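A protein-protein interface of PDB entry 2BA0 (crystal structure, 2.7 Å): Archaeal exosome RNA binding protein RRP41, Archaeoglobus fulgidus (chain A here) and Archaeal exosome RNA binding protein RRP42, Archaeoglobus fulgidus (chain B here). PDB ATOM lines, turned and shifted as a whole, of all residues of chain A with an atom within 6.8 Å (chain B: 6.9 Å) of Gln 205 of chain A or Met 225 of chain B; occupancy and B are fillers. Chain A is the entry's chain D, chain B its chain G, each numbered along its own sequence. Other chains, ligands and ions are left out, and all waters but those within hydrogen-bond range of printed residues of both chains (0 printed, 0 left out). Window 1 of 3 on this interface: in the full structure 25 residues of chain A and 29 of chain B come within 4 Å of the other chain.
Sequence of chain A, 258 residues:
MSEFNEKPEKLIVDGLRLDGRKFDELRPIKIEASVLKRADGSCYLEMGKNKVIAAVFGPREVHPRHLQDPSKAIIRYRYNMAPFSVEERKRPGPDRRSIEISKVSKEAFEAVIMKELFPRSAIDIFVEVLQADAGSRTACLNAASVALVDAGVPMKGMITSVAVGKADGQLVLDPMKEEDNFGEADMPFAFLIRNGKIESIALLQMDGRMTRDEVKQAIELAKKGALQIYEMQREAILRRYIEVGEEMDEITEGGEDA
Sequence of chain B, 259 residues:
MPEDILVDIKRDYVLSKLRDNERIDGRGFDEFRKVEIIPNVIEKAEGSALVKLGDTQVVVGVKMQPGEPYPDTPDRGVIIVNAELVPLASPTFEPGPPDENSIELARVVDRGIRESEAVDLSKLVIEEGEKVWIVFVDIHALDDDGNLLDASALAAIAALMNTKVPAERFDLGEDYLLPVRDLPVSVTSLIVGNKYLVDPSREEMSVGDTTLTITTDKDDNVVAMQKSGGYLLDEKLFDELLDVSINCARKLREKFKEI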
ATOM      1  N   GLU A 100      19.470 -10.379 -26.140  1.00  0.00           N
ATOM      2  CA  GLU A 100      20.089  -9.096 -26.429  1.00  0.00           C
ATOM      3  C   GLU A 100      21.570  -9.105 -26.062  1.00  0.00           C
ATOM      4  O   GLU A 100      22.405  -8.548 -26.780  1.00  0.00           O
ATOM      5  CB  GLU A 100      19.369  -7.970 -25.694  1.00  0.00           C
ATOM      6  CG  GLU A 100      19.439  -6.655 -26.452  1.00  0.00           C
ATOM      7  CD  GLU A 100      19.773  -5.476 -25.556  1.00  0.00           C
ATOM      8  OE1 GLU A 100      18.849  -4.911 -24.908  1.00  0.00           O
ATOM      9  OE2 GLU A 100      20.979  -5.124 -25.496  1.00  0.00           O
ATOM     10  N   ILE A 101      21.908  -9.737 -24.947  1.00  0.00           N
ATOM     11  CA  ILE A 101      23.303  -9.801 -24.554  1.00  0.00           C
ATOM     12  C   ILE A 101      24.078 -10.590 -25.610  1.00  0.00           C
ATOM     13  O   ILE A 101      25.145 -10.159 -26.056  1.00  0.00           O
ATOM     14  CB  ILE A 101      23.457 -10.464 -23.175  1.00  0.00           C
ATOM     15  CG1 ILE A 101      22.958  -9.497 -22.106  1.00  0.00           C
ATOM     16  CG2 ILE A 101      24.911 -10.863 -22.923  1.00  0.00           C
ATOM     17  CD1 ILE A 101      22.932 -10.089 -20.717  1.00  0.00           C
ATOM     18  N   VAL A 104      24.706  -8.227 -28.848  1.00  0.00           N
ATOM     19  CA  VAL A 104      25.678  -7.159 -28.682  1.00  0.00           C
ATOM     20  C   VAL A 104      27.090  -7.745 -28.503  1.00  0.00           C
ATOM     21  O   VAL A 104      28.074  -7.151 -28.932  1.00  0.00           O
ATOM     22  CB  VAL A 104      25.270  -6.268 -27.474  1.00  0.00           C
ATOM     23  CG1 VAL A 104      25.266  -7.089 -26.198  1.00  0.00           C
ATOM     24  CG2 VAL A 104      26.194  -5.097 -27.342  1.00  0.00           C
ATOM     25  N   ARG A 137      27.784 -10.014 -17.864  1.00  0.00           N
ATOM     26  CA  ARG A 137      27.871  -9.675 -19.283  1.00  0.00           C
ATOM     27  C   ARG A 137      29.330  -9.346 -19.602  1.00  0.00           C
ATOM     28  O   ARG A 137      29.911  -9.851 -20.560  1.00  0.00           O
ATOM     29  CB  ARG A 137      26.991  -8.453 -19.539  1.00  0.00           C
ATOM     30  CG  ARG A 137      27.120  -7.840 -20.890  1.00  0.00           C
ATOM     31  CD  ARG A 137      26.337  -6.546 -20.941  1.00  0.00           C
ATOM     32  NE  ARG A 137      25.041  -6.696 -20.296  1.00  0.00           N
ATOM     33  CZ  ARG A 137      23.955  -6.022 -20.650  1.00  0.00           C
ATOM     34  NH1 ARG A 137      22.805  -6.215 -20.013  1.00  0.00           N
ATOM     35  NH2 ARG A 137      24.018  -5.161 -21.655  1.00  0.00           N
ATOM     36  N   ASP A 186      24.179   2.579 -15.064  1.00  0.00           N
ATOM     37  CA  ASP A 186      25.034   1.422 -15.309  1.00  0.00           C
ATOM     38  C   ASP A 186      25.451   1.545 -16.760  1.00  0.00           C
ATOM     39  O   ASP A 186      24.600   1.677 -17.641  1.00  0.00           O
ATOM     40  CB  ASP A 186      24.281   0.105 -15.111  1.00  0.00           C
ATOM     41  CG  ASP A 186      25.133  -1.109 -15.446  1.00  0.00           C
ATOM     42  N   MET A 187      26.752   1.488 -17.017  1.00  0.00           N
ATOM     43  CA  MET A 187      27.244   1.644 -18.376  1.00  0.00           C
ATOM     44  C   MET A 187      28.362   0.679 -18.742  1.00  0.00           C
ATOM     45  O   MET A 187      29.532   0.984 -18.559  1.00  0.00           O
ATOM     46  CB  MET A 187      27.724   3.080 -18.556  1.00  0.00           C
ATOM     47  CG  MET A 187      28.168   3.428 -19.948  1.00  0.00           C
ATOM     48  SD  MET A 187      28.588   5.172 -20.070  1.00  0.00           S
ATOM     49  CE  MET A 187      28.213   5.485 -21.788  1.00  0.00           C
ATOM     50  N   PRO A 188      28.013  -0.501 -19.278  1.00  0.00           N
ATOM     51  CA  PRO A 188      29.038  -1.477 -19.655  1.00  0.00           C
ATOM     52  C   PRO A 188      29.767  -1.067 -20.930  1.00  0.00           C
ATOM     53  O   PRO A 188      29.135  -0.607 -21.870  1.00  0.00           O
ATOM     54  CB  PRO A 188      28.233  -2.764 -19.826  1.00  0.00           C
ATOM     55  CG  PRO A 188      26.916  -2.272 -20.330  1.00  0.00           C
ATOM     56  CD  PRO A 188      26.655  -1.045 -19.489  1.00  0.00           C
ATOM     57  N   PHE A 189      31.092  -1.214 -20.942  1.00  0.00           N
ATOM     58  CA  PHE A 189      31.927  -0.875 -22.100  1.00  0.00           C
ATOM     59  C   PHE A 189      32.781  -2.066 -22.522  1.00  0.00           C
ATOM     60  O   PHE A 189      33.020  -2.991 -21.731  1.00  0.00           O
ATOM     61  CB  PHE A 189      32.927   0.247 -21.783  1.00  0.00           C
ATOM     62  CG  PHE A 189      32.333   1.617 -21.698  1.00  0.00           C
ATOM     63  CD1 PHE A 189      31.907   2.135 -20.480  1.00  0.00           C
ATOM     64  CD2 PHE A 189      32.255   2.421 -22.829  1.00  0.00           C
ATOM     65  CE1 PHE A 189      31.416   3.442 -20.383  1.00  0.00           C
ATOM     66  CE2 PHE A 189      31.764   3.732 -22.747  1.00  0.00           C
ATOM     67  CZ  PHE A 189      31.345   4.242 -21.516  1.00  0.00           C
ATOM     68  N   ILE A 201      36.238   1.556 -29.407  1.00  0.00           N
ATOM     69  CA  ILE A 201      35.265   0.824 -28.609  1.00  0.00           C
ATOM     70  C   ILE A 201      34.524  -0.234 -29.446  1.00  0.00           C
ATOM     71  O   ILE A 201      34.174  -0.001 -30.611  1.00  0.00           O
ATOM     72  CB  ILE A 201      34.241   1.773 -27.932  1.00  0.00           C
ATOM     73  CG1 ILE A 201      32.891   1.649 -28.620  1.00  0.00           C
ATOM     74  CG2 ILE A 201      34.730   3.218 -27.979  1.00  0.00           C
ATOM     75  CD1 ILE A 201      31.814   2.384 -27.923  1.00  0.00           C
ATOM     76  N   LEU A 203      31.954  -2.229 -27.804  1.00  0.00           N
ATOM     77  CA  LEU A 203      30.636  -2.351 -27.178  1.00  0.00           C
ATOM     78  C   LEU A 203      30.377  -1.156 -26.258  1.00  0.00           C
ATOM     79  O   LEU A 203      31.219  -0.792 -25.447  1.00  0.00           O
ATOM     80  CB  LEU A 203      30.521  -3.675 -26.392  1.00  0.00           C
ATOM     81  CG  LEU A 203      29.230  -3.978 -25.596  1.00  0.00           C
ATOM     82  CD1 LEU A 203      29.062  -5.486 -25.417  1.00  0.00           C
ATOM     83  CD2 LEU A 203      29.259  -3.269 -24.249  1.00  0.00           C
ATOM     84  N   LEU A 204      29.208  -0.545 -26.413  1.00  0.00           N
ATOM     85  CA  LEU A 204      28.816   0.603 -25.619  1.00  0.00           C
ATOM     86  C   LEU A 204      27.308   0.557 -25.393  1.00  0.00           C
ATOM     87  O   LEU A 204      26.532   0.611 -26.342  1.00  0.00           O
ATOM     88  CB  LEU A 204      29.174   1.899 -26.344  1.00  0.00           C
ATOM     89  CG  LEU A 204      29.177   3.226 -25.550  1.00  0.00           C
ATOM     90  CD1 LEU A 204      29.705   4.340 -26.453  1.00  0.00           C
ATOM     91  CD2 LEU A 204      27.779   3.589 -25.059  1.00  0.00           C
ATOM     92  N   GLN A 205      26.908   0.455 -24.132  1.00  0.00           N
ATOM     93  CA  GLN A 205      25.502   0.428 -23.747  1.00  0.00           C
ATOM     94  C   GLN A 205      25.361   1.274 -22.498  1.00  0.00           C
ATOM     95  O   GLN A 205      26.306   1.387 -21.720  1.00  0.00           O
ATOM     96  CB  GLN A 205      25.049  -0.992 -23.416  1.00  0.00           C
ATOM     97  CG  GLN A 205      24.662  -1.835 -24.597  1.00  0.00           C
ATOM     98  CD  GLN A 205      24.036  -3.157 -24.179  1.00  0.00           C
ATOM     99  OE1 GLN A 205      24.721  -4.050 -23.676  1.00  0.00           O
ATOM    100  NE2 GLN A 205      22.725  -3.285 -24.378  1.00  0.00           N
ATOM    101  N   MET A 206      24.184   1.852 -22.289  1.00  0.00           N
ATOM    102  CA  MET A 206      23.970   2.668 -21.106  1.00  0.00           C
ATOM    103  C   MET A 206      22.502   2.870 -20.758  1.00  0.00           C
ATOM    104  O   MET A 206      21.671   3.146 -21.624  1.00  0.00           O
ATOM    105  CB  MET A 206      24.661   4.026 -21.282  1.00  0.00           C
ATOM    106  CG  MET A 206      24.461   5.011 -20.139  1.00  0.00           C
ATOM    107  SD  MET A 206      22.932   5.963 -20.265  1.00  0.00           S
ATOM    108  CE  MET A 206      22.946   6.832 -18.656  1.00  0.00           C
ATOM    109  N   ASP A 207      22.209   2.708 -19.472  1.00  0.00           N
ATOM    110  CA  ASP A 207      20.882   2.898 -18.912  1.00  0.00           C
ATOM    111  C   ASP A 207      21.065   3.749 -17.672  1.00  0.00           C
ATOM    112  O   ASP A 207      21.940   3.477 -16.843  1.00  0.00           O
ATOM    113  CB  ASP A 207      20.240   1.571 -18.501  1.00  0.00           C
ATOM    114  CG  ASP A 207      19.502   0.899 -19.645  1.00  0.00           C
ATOM    115  OD1 ASP A 207      20.163   0.447 -20.602  1.00  0.00           O
ATOM    116  OD2 ASP A 207      18.252   0.822 -19.598  1.00  0.00           O
ATOM    117  N   GLY A 208      20.254   4.787 -17.539  1.00  0.00           N
ATOM    118  CA  GLY A 208      20.373   5.613 -16.359  1.00  0.00           C
ATOM    119  C   GLY A 208      20.050   7.059 -16.617  1.00  0.00           C
ATOM    120  O   GLY A 208      19.159   7.387 -17.386  1.00  0.00           O
ATOM    121  N   VAL A 215      29.311  11.335 -18.801  1.00  0.00           N
ATOM    122  CA  VAL A 215      29.504  10.271 -19.774  1.00  0.00           C
ATOM    123  C   VAL A 215      30.977  10.240 -20.207  1.00  0.00           C
ATOM    124  O   VAL A 215      31.598   9.170 -20.267  1.00  0.00           O
ATOM    125  CB  VAL A 215      28.585  10.476 -21.007  1.00  0.00           C
ATOM    126  CG1 VAL A 215      28.851   9.424 -22.049  1.00  0.00           C
ATOM    127  CG2 VAL A 215      27.137  10.412 -20.577  1.00  0.00           C
ATOM    128  N   GLU B 104      15.322  -6.004 -29.970  1.00  0.00           N
ATOM    129  CA  GLU B 104      16.220  -4.913 -29.622  1.00  0.00           C
ATOM    130  C   GLU B 104      15.591  -3.525 -29.814  1.00  0.00           C
ATOM    131  O   GLU B 104      15.869  -2.603 -29.043  1.00  0.00           O
ATOM    132  CB  GLU B 104      17.515  -5.023 -30.428  1.00  0.00           C
ATOM    133  CG  GLU B 104      18.478  -3.861 -30.202  1.00  0.00           C
ATOM    134  CD  GLU B 104      19.890  -4.157 -30.674  1.00  0.00           C
ATOM    135  OE1 GLU B 104      20.594  -4.947 -30.005  1.00  0.00           O
ATOM    136  OE2 GLU B 104      20.294  -3.598 -31.717  1.00  0.00           O
ATOM    137  N   ARG B 107      13.459  -3.027 -26.801  1.00  0.00           N
ATOM    138  CA  ARG B 107      14.189  -2.760 -25.570  1.00  0.00           C
ATOM    139  C   ARG B 107      14.655  -1.315 -25.483  1.00  0.00           C
ATOM    140  O   ARG B 107      14.579  -0.701 -24.424  1.00  0.00           O
ATOM    141  CB  ARG B 107      15.385  -3.688 -25.421  1.00  0.00           C
ATOM    142  CG  ARG B 107      15.030  -5.136 -25.232  1.00  0.00           C
ATOM    143  CD  ARG B 107      16.161  -5.867 -24.501  1.00  0.00           C
ATOM    144  NE  ARG B 107      15.776  -6.244 -23.139  1.00  0.00           N
ATOM    145  CZ  ARG B 107      16.613  -6.333 -22.115  1.00  0.00           C
ATOM    146  NH1 ARG B 107      16.150  -6.688 -20.927  1.00  0.00           N
ATOM    147  NH2 ARG B 107      17.904  -6.053 -22.269  1.00  0.00           N
ATOM    148  N   VAL B 108      15.129  -0.761 -26.589  1.00  0.00           N
ATOM    149  CA  VAL B 108      15.591   0.613 -26.552  1.00  0.00           C
ATOM    150  C   VAL B 108      14.427   1.545 -26.265  1.00  0.00           C
ATOM    151  O   VAL B 108      14.520   2.395 -25.382  1.00  0.00           O
ATOM    152  CB  VAL B 108      16.275   1.033 -27.873  1.00  0.00           C
ATOM    153  CG1 VAL B 108      16.659   2.509 -27.800  1.00  0.00           C
ATOM    154  CG2 VAL B 108      17.525   0.166 -28.124  1.00  0.00           C
ATOM    155  N   ARG B 111      13.765   1.392 -22.726  1.00  0.00           N
ATOM    156  CA  ARG B 111      14.769   1.927 -21.812  1.00  0.00           C
ATOM    157  C   ARG B 111      14.681   3.430 -21.631  1.00  0.00           C
ATOM    158  O   ARG B 111      14.929   3.934 -20.532  1.00  0.00           O
ATOM    159  CB  ARG B 111      16.183   1.546 -22.285  1.00  0.00           C
ATOM    160  CG  ARG B 111      16.506   0.079 -22.120  1.00  0.00           C
ATOM    161  CD  ARG B 111      17.581  -0.360 -23.085  1.00  0.00           C
ATOM    162  NE  ARG B 111      18.849   0.316 -22.845  1.00  0.00           N
ATOM    163  CZ  ARG B 111      19.909   0.201 -23.640  1.00  0.00           C
ATOM    164  NH1 ARG B 111      21.031   0.847 -23.357  1.00  0.00           N
ATOM    165  NH2 ARG B 111      19.841  -0.552 -24.729  1.00  0.00           N
ATOM    166  N   LEU B 212      24.686   3.858 -33.816  1.00  0.00           N
ATOM    167  CA  LEU B 212      24.860   4.319 -32.459  1.00  0.00           C
ATOM    168  C   LEU B 212      23.599   5.115 -32.155  1.00  0.00           C
ATOM    169  O   LEU B 212      23.226   6.008 -32.912  1.00  0.00           O
ATOM    170  CB  LEU B 212      26.105   5.210 -32.374  1.00  0.00           C
ATOM    171  CG  LEU B 212      26.554   5.820 -31.043  1.00  0.00           C
ATOM    172  CD1 LEU B 212      25.620   6.926 -30.705  1.00  0.00           C
ATOM    173  CD2 LEU B 212      26.577   4.783 -29.933  1.00  0.00           C
ATOM    174  N   THR B 213      22.927   4.763 -31.062  1.00  0.00           N
ATOM    175  CA  THR B 213      21.710   5.449 -30.664  1.00  0.00           C
ATOM    176  C   THR B 213      21.890   6.052 -29.280  1.00  0.00           C
ATOM    177  O   THR B 213      22.325   5.367 -28.358  1.00  0.00           O
ATOM    178  CB  THR B 213      20.532   4.485 -30.618  1.00  0.00           C
ATOM    179  OG1 THR B 213      20.512   3.713 -31.819  1.00  0.00           O
ATOM    180  CG2 THR B 213      19.223   5.248 -30.517  1.00  0.00           C
ATOM    181  N   ILE B 214      21.560   7.334 -29.147  1.00  0.00           N
ATOM    182  CA  ILE B 214      21.662   8.045 -27.875  1.00  0.00           C
ATOM    183  C   ILE B 214      20.297   8.632 -27.521  1.00  0.00           C
ATOM    184  O   ILE B 214      19.717   9.345 -28.333  1.00  0.00           O
ATOM    185  CB  ILE B 214      22.648   9.215 -27.974  1.00  0.00           C
ATOM    186  CG1 ILE B 214      24.025   8.705 -28.387  1.00  0.00           C
ATOM    187  CG2 ILE B 214      22.731   9.936 -26.654  1.00  0.00           C
ATOM    188  CD1 ILE B 214      25.029   9.811 -28.608  1.00  0.00           C
ATOM    189  N   THR B 215      19.789   8.340 -26.324  1.00  0.00           N
ATOM    190  CA  THR B 215      18.497   8.867 -25.899  1.00  0.00           C
ATOM    191  C   THR B 215      18.655   9.897 -24.765  1.00  0.00           C
ATOM    192  O   THR B 215      19.337   9.666 -23.765  1.00  0.00           O
ATOM    193  CB  THR B 215      17.542   7.731 -25.440  1.00  0.00           C
ATOM    194  OG1 THR B 215      17.433   6.750 -26.472  1.00  0.00           O
ATOM    195  CG2 THR B 215      16.149   8.280 -25.179  1.00  0.00           C
ATOM    196  N   VAL B 222      21.781  12.435 -20.802  1.00  0.00           N
ATOM    197  CA  VAL B 222      21.752  11.166 -21.515  1.00  0.00           C
ATOM    198  C   VAL B 222      21.030  10.212 -20.568  1.00  0.00           C
ATOM    199  O   VAL B 222      21.242  10.252 -19.353  1.00  0.00           O
ATOM    200  CB  VAL B 222      23.167  10.660 -21.806  1.00  0.00           C
ATOM    201  CG1 VAL B 222      23.109   9.308 -22.481  1.00  0.00           C
ATOM    202  CG2 VAL B 222      23.884  11.664 -22.691  1.00  0.00           C
ATOM    203  N   VAL B 223      20.179   9.357 -21.114  1.00  0.00           N
ATOM    204  CA  VAL B 223      19.401   8.465 -20.282  1.00  0.00           C
ATOM    205  C   VAL B 223      19.453   7.036 -20.791  1.00  0.00           C
ATOM    206  O   VAL B 223      19.086   6.098 -20.088  1.00  0.00           O
ATOM    207  CB  VAL B 223      17.936   9.009 -20.204  1.00  0.00           C
ATOM    208  CG1 VAL B 223      16.977   8.115 -20.966  1.00  0.00           C
ATOM    209  CG2 VAL B 223      17.523   9.189 -18.758  1.00  0.00           C
ATOM    210  N   ALA B 224      19.908   6.883 -22.029  1.00  0.00           N
ATOM    211  CA  ALA B 224      20.050   5.569 -22.660  1.00  0.00           C
ATOM    212  C   ALA B 224      20.952   5.682 -23.878  1.00  0.00           C
ATOM    213  O   ALA B 224      20.829   6.626 -24.659  1.00  0.00           O
ATOM    214  CB  ALA B 224      18.692   5.019 -23.074  1.00  0.00           C
ATOM    215  N   MET B 225      21.873   4.730 -24.018  1.00  0.00           N
ATOM    216  CA  MET B 225      22.795   4.690 -25.155  1.00  0.00           C
ATOM    217  C   MET B 225      22.917   3.259 -25.640  1.00  0.00           C
ATOM    218  O   MET B 225      22.849   2.329 -24.839  1.00  0.00           O
ATOM    219  CB  MET B 225      24.178   5.211 -24.775  1.00  0.00           C
ATOM    220  CG  MET B 225      24.206   6.672 -24.394  1.00  0.00           C
ATOM    221  SD  MET B 225      25.890   7.253 -24.238  1.00  0.00           S
ATOM    222  CE  MET B 225      26.129   7.841 -25.866  1.00  0.00           C
ATOM    223  N   GLN B 226      23.105   3.083 -26.942  1.00  0.00           N
ATOM    224  CA  GLN B 226      23.203   1.745 -27.504  1.00  0.00           C
ATOM    225  C   GLN B 226      23.966   1.700 -28.824  1.00  0.00           C
ATOM    226  O   GLN B 226      23.547   2.299 -29.818  1.00  0.00           O
ATOM    227  CB  GLN B 226      21.792   1.188 -27.718  1.00  0.00           C
ATOM    228  CG  GLN B 226      21.735  -0.206 -28.304  1.00  0.00           C
ATOM    229  CD  GLN B 226      22.156  -1.281 -27.314  1.00  0.00           C
ATOM    230  OE1 GLN B 226      22.687  -2.314 -27.710  1.00  0.00           O
ATOM    231  N   LYS B 227      25.094   1.000 -28.827  1.00  0.00           N
ATOM    232  CA  LYS B 227      25.886   0.840 -30.039  1.00  0.00           C
ATOM    233  C   LYS B 227      25.449  -0.496 -30.631  1.00  0.00           C
ATOM    234  O   LYS B 227      25.287  -1.467 -29.895  1.00  0.00           O
ATOM    235  CB  LYS B 227      27.382   0.817 -29.709  1.00  0.00           C
ATOM    236  CG  LYS B 227      28.258   0.271 -30.825  1.00  0.00           C
ATOM    237  CD  LYS B 227      29.714   0.671 -30.644  1.00  0.00           C
ATOM    238  CE  LYS B 227      30.664  -0.494 -30.799  1.00  0.00           C
ATOM    239  NZ  LYS B 227      30.205  -1.502 -31.798  1.00  0.00           N
ATOM    240  N   PHE B 238      32.682   9.520 -31.250  1.00  0.00           N
ATOM    241  CA  PHE B 238      31.712   9.448 -30.170  1.00  0.00           C
ATOM    242  C   PHE B 238      31.572  10.804 -29.455  1.00  0.00           C
ATOM    243  O   PHE B 238      30.459  11.252 -29.168  1.00  0.00           O
ATOM    244  CB  PHE B 238      32.131   8.390 -29.153  1.00  0.00           C
ATOM    245  CG  PHE B 238      31.215   8.300 -27.980  1.00  0.00           C
ATOM    246  CD1 PHE B 238      29.984   7.670 -28.094  1.00  0.00           C
ATOM    247  CD2 PHE B 238      31.557   8.883 -26.769  1.00  0.00           C
ATOM    248  CE1 PHE B 238      29.105   7.622 -27.019  1.00  0.00           C
ATOM    249  CE2 PHE B 238      30.679   8.842 -25.685  1.00  0.00           C
ATOM    250  CZ  PHE B 238      29.451   8.209 -25.816  1.00  0.00           C
ATOM    251  N   LEU B 242      28.016  12.596 -29.641  1.00  0.00           N
ATOM    252  CA  LEU B 242      27.302  12.736 -28.385  1.00  0.00           C
ATOM    253  C   LEU B 242      26.643  14.108 -28.316  1.00  0.00           C
ATOM    254  O   LEU B 242      25.453  14.226 -28.045  1.00  0.00           O
ATOM    255  CB  LEU B 242      28.266  12.589 -27.207  1.00  0.00           C
ATOM    256  CG  LEU B 242      27.710  12.059 -25.885  1.00  0.00           C
ATOM    257  CD1 LEU B 242      28.306  12.871 -24.757  1.00  0.00           C
ATOM    258  CD2 LEU B 242      26.194  12.128 -25.860  1.00  0.00           C
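Of the printed residues of chain B, Gln 205 of chain A touches Arg 111, Met 225 and Gln 226.
Of chain A, only Met 187, Leu 204, Gln 205 and Met 206 come within 4 Å of Met 225 of chain B.
Printed residues of chain B within 4 Å of Asp 207 of chain A: Arg 111 (2.6 Å) and Val 223 (3.9 Å).
Of the printed residues of chain A, Arg 107 of chain B touches Glu 100.
Of the printed residues of chain A, Ala 224 of chain B touches Met 206.
Printed residues of chain A within 4 Å of Gln 226 of chain B: Glu 100 (3.96 Å), Leu 204 (3.7 Å) and Gln 205 (3.5 Å).
Of the printed residues of chain A, Lys 227 of chain B touches Ile 201 (3.5 Å), Leu 203 (3.7 Å) and Leu 204 (2.9 Å).
Ile 101 of chain A touches none of the printed residues of chain B.
Val 104 of chain A touches none of the printed residues of chain B.
The nearest printed residue of chain B that does not touch Gln 205 of chain A is Lys 227 of chain B (5.1 Å).
The nearest residue of chain A that does not touch Met 225 of chain B is Val 215 of chain A (4.3 Å).
The nearest printed residue of chain A that does not touch Arg 111 of chain B is Glu 100 of chain A (4.5 Å).
CE of Met 187 of chain A touches SD of Met 225 of chain B (3.8 Å).
Ile 201 of chain A touches Lys 227 of chain B.
Lys 227 of chain B touches Leu 203 of chain A.
Met 225 of chain B touches Leu 204 of chain A (CB to CD2, 3.96 Å).
O of Leu 204 of chain A touches CA of Gln 226 of chain B (3.7 Å).
Leu 204 of chain A touches Phe 238 of chain B.
Arg 111 of chain B touches Gln 205 of chain A.
CA of Gln 205 of chain A touches O of Met 225 of chain B, 3.4 Å away.
Met 206 of chain A touches Val 222 of chain B (CE to O, 3.9 Å).
Val 223 of chain B touches Asp 207 of chain A.
The guanidinium group (NH2) of Arg 107 of chain B lies within salt-bridge range of the side-chain carboxylate (OE1) of Glu 100 of chain A, 3.0 Å away.
The backbone NH (N) of Lys 227 of chain B is in hydrogen-bond range of the backbone carbonyl oxygen (O) of Leu 204 of chain A (2.9 Å).
OE1 of Gln 226 of chain B lies within hydrogen-bond range of NE2 of Gln 205 of chain A, at 3.5 Å.
NH1 of Arg 111 of chain B lies within hydrogen-bond range of O of Met 206 of chain A (2.9 Å).
SD of Met 206 of chain A sits at hydrogen-bond distance from N of Ala 224 of chain B, 3.6 Å away.
The backbone carbonyl oxygen of Met 206 of chain A sits at hydrogen-bond distance from the backbone NH of Met 225 of chain B (2.9 Å).
The side-chain carboxylate of Asp 207 of chain A lies within salt-bridge range of the guanidinium group of Arg 111 of chain B (2.6 Å).
The backbone carbonyl oxygen (O) of Val 223 of chain B is in hydrogen-bond range of the backbone NH (N) of Gly 208 of chain A.
OE2 of Glu 100 of chain A sits at hydrogen-bond distance from NE2 of Gln 205 of chain A (2.8 Å).
The backbone NH of Gln 205 of chain A lies within hydrogen-bond range of the backbone carbonyl oxygen of Pro 188 of chain A (3.3 Å).
NH1 of Arg 111 of chain B lies within hydrogen-bond range of O of Met 225 of chain B.
O of Thr 213 of chain B lies within hydrogen-bond range of N of Gln 226 of chain B (2.8 Å).
N of Val 223 of chain B lies within hydrogen-bond range of O of Thr 215 of chain B.
The backbone NH of Thr 215 of chain B lies within hydrogen-bond range of the backbone carbonyl oxygen of Ala 224 of chain B (2.6 Å).
Of the 16 printed residues of chain B, 9 touch a printed residue of chain A.
Along chain B the printed residues that touch a printed residue of chain A span positions 107 to 238.
Hydrophobic or aromatic side chains of chain A that line the printed part of chain B: Met 187, Ile 201, Leu 204 and Met 206.
Among the printed residues, Asp or Glu carboxylates within 4 Å of a Lys or Arg side-chain nitrogen of the other chain: Glu 100 of chain A with Arg 107 of chain B (3.0 Å) and Asp 207 of chain A with Arg 111 of chain B (2.6 Å).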
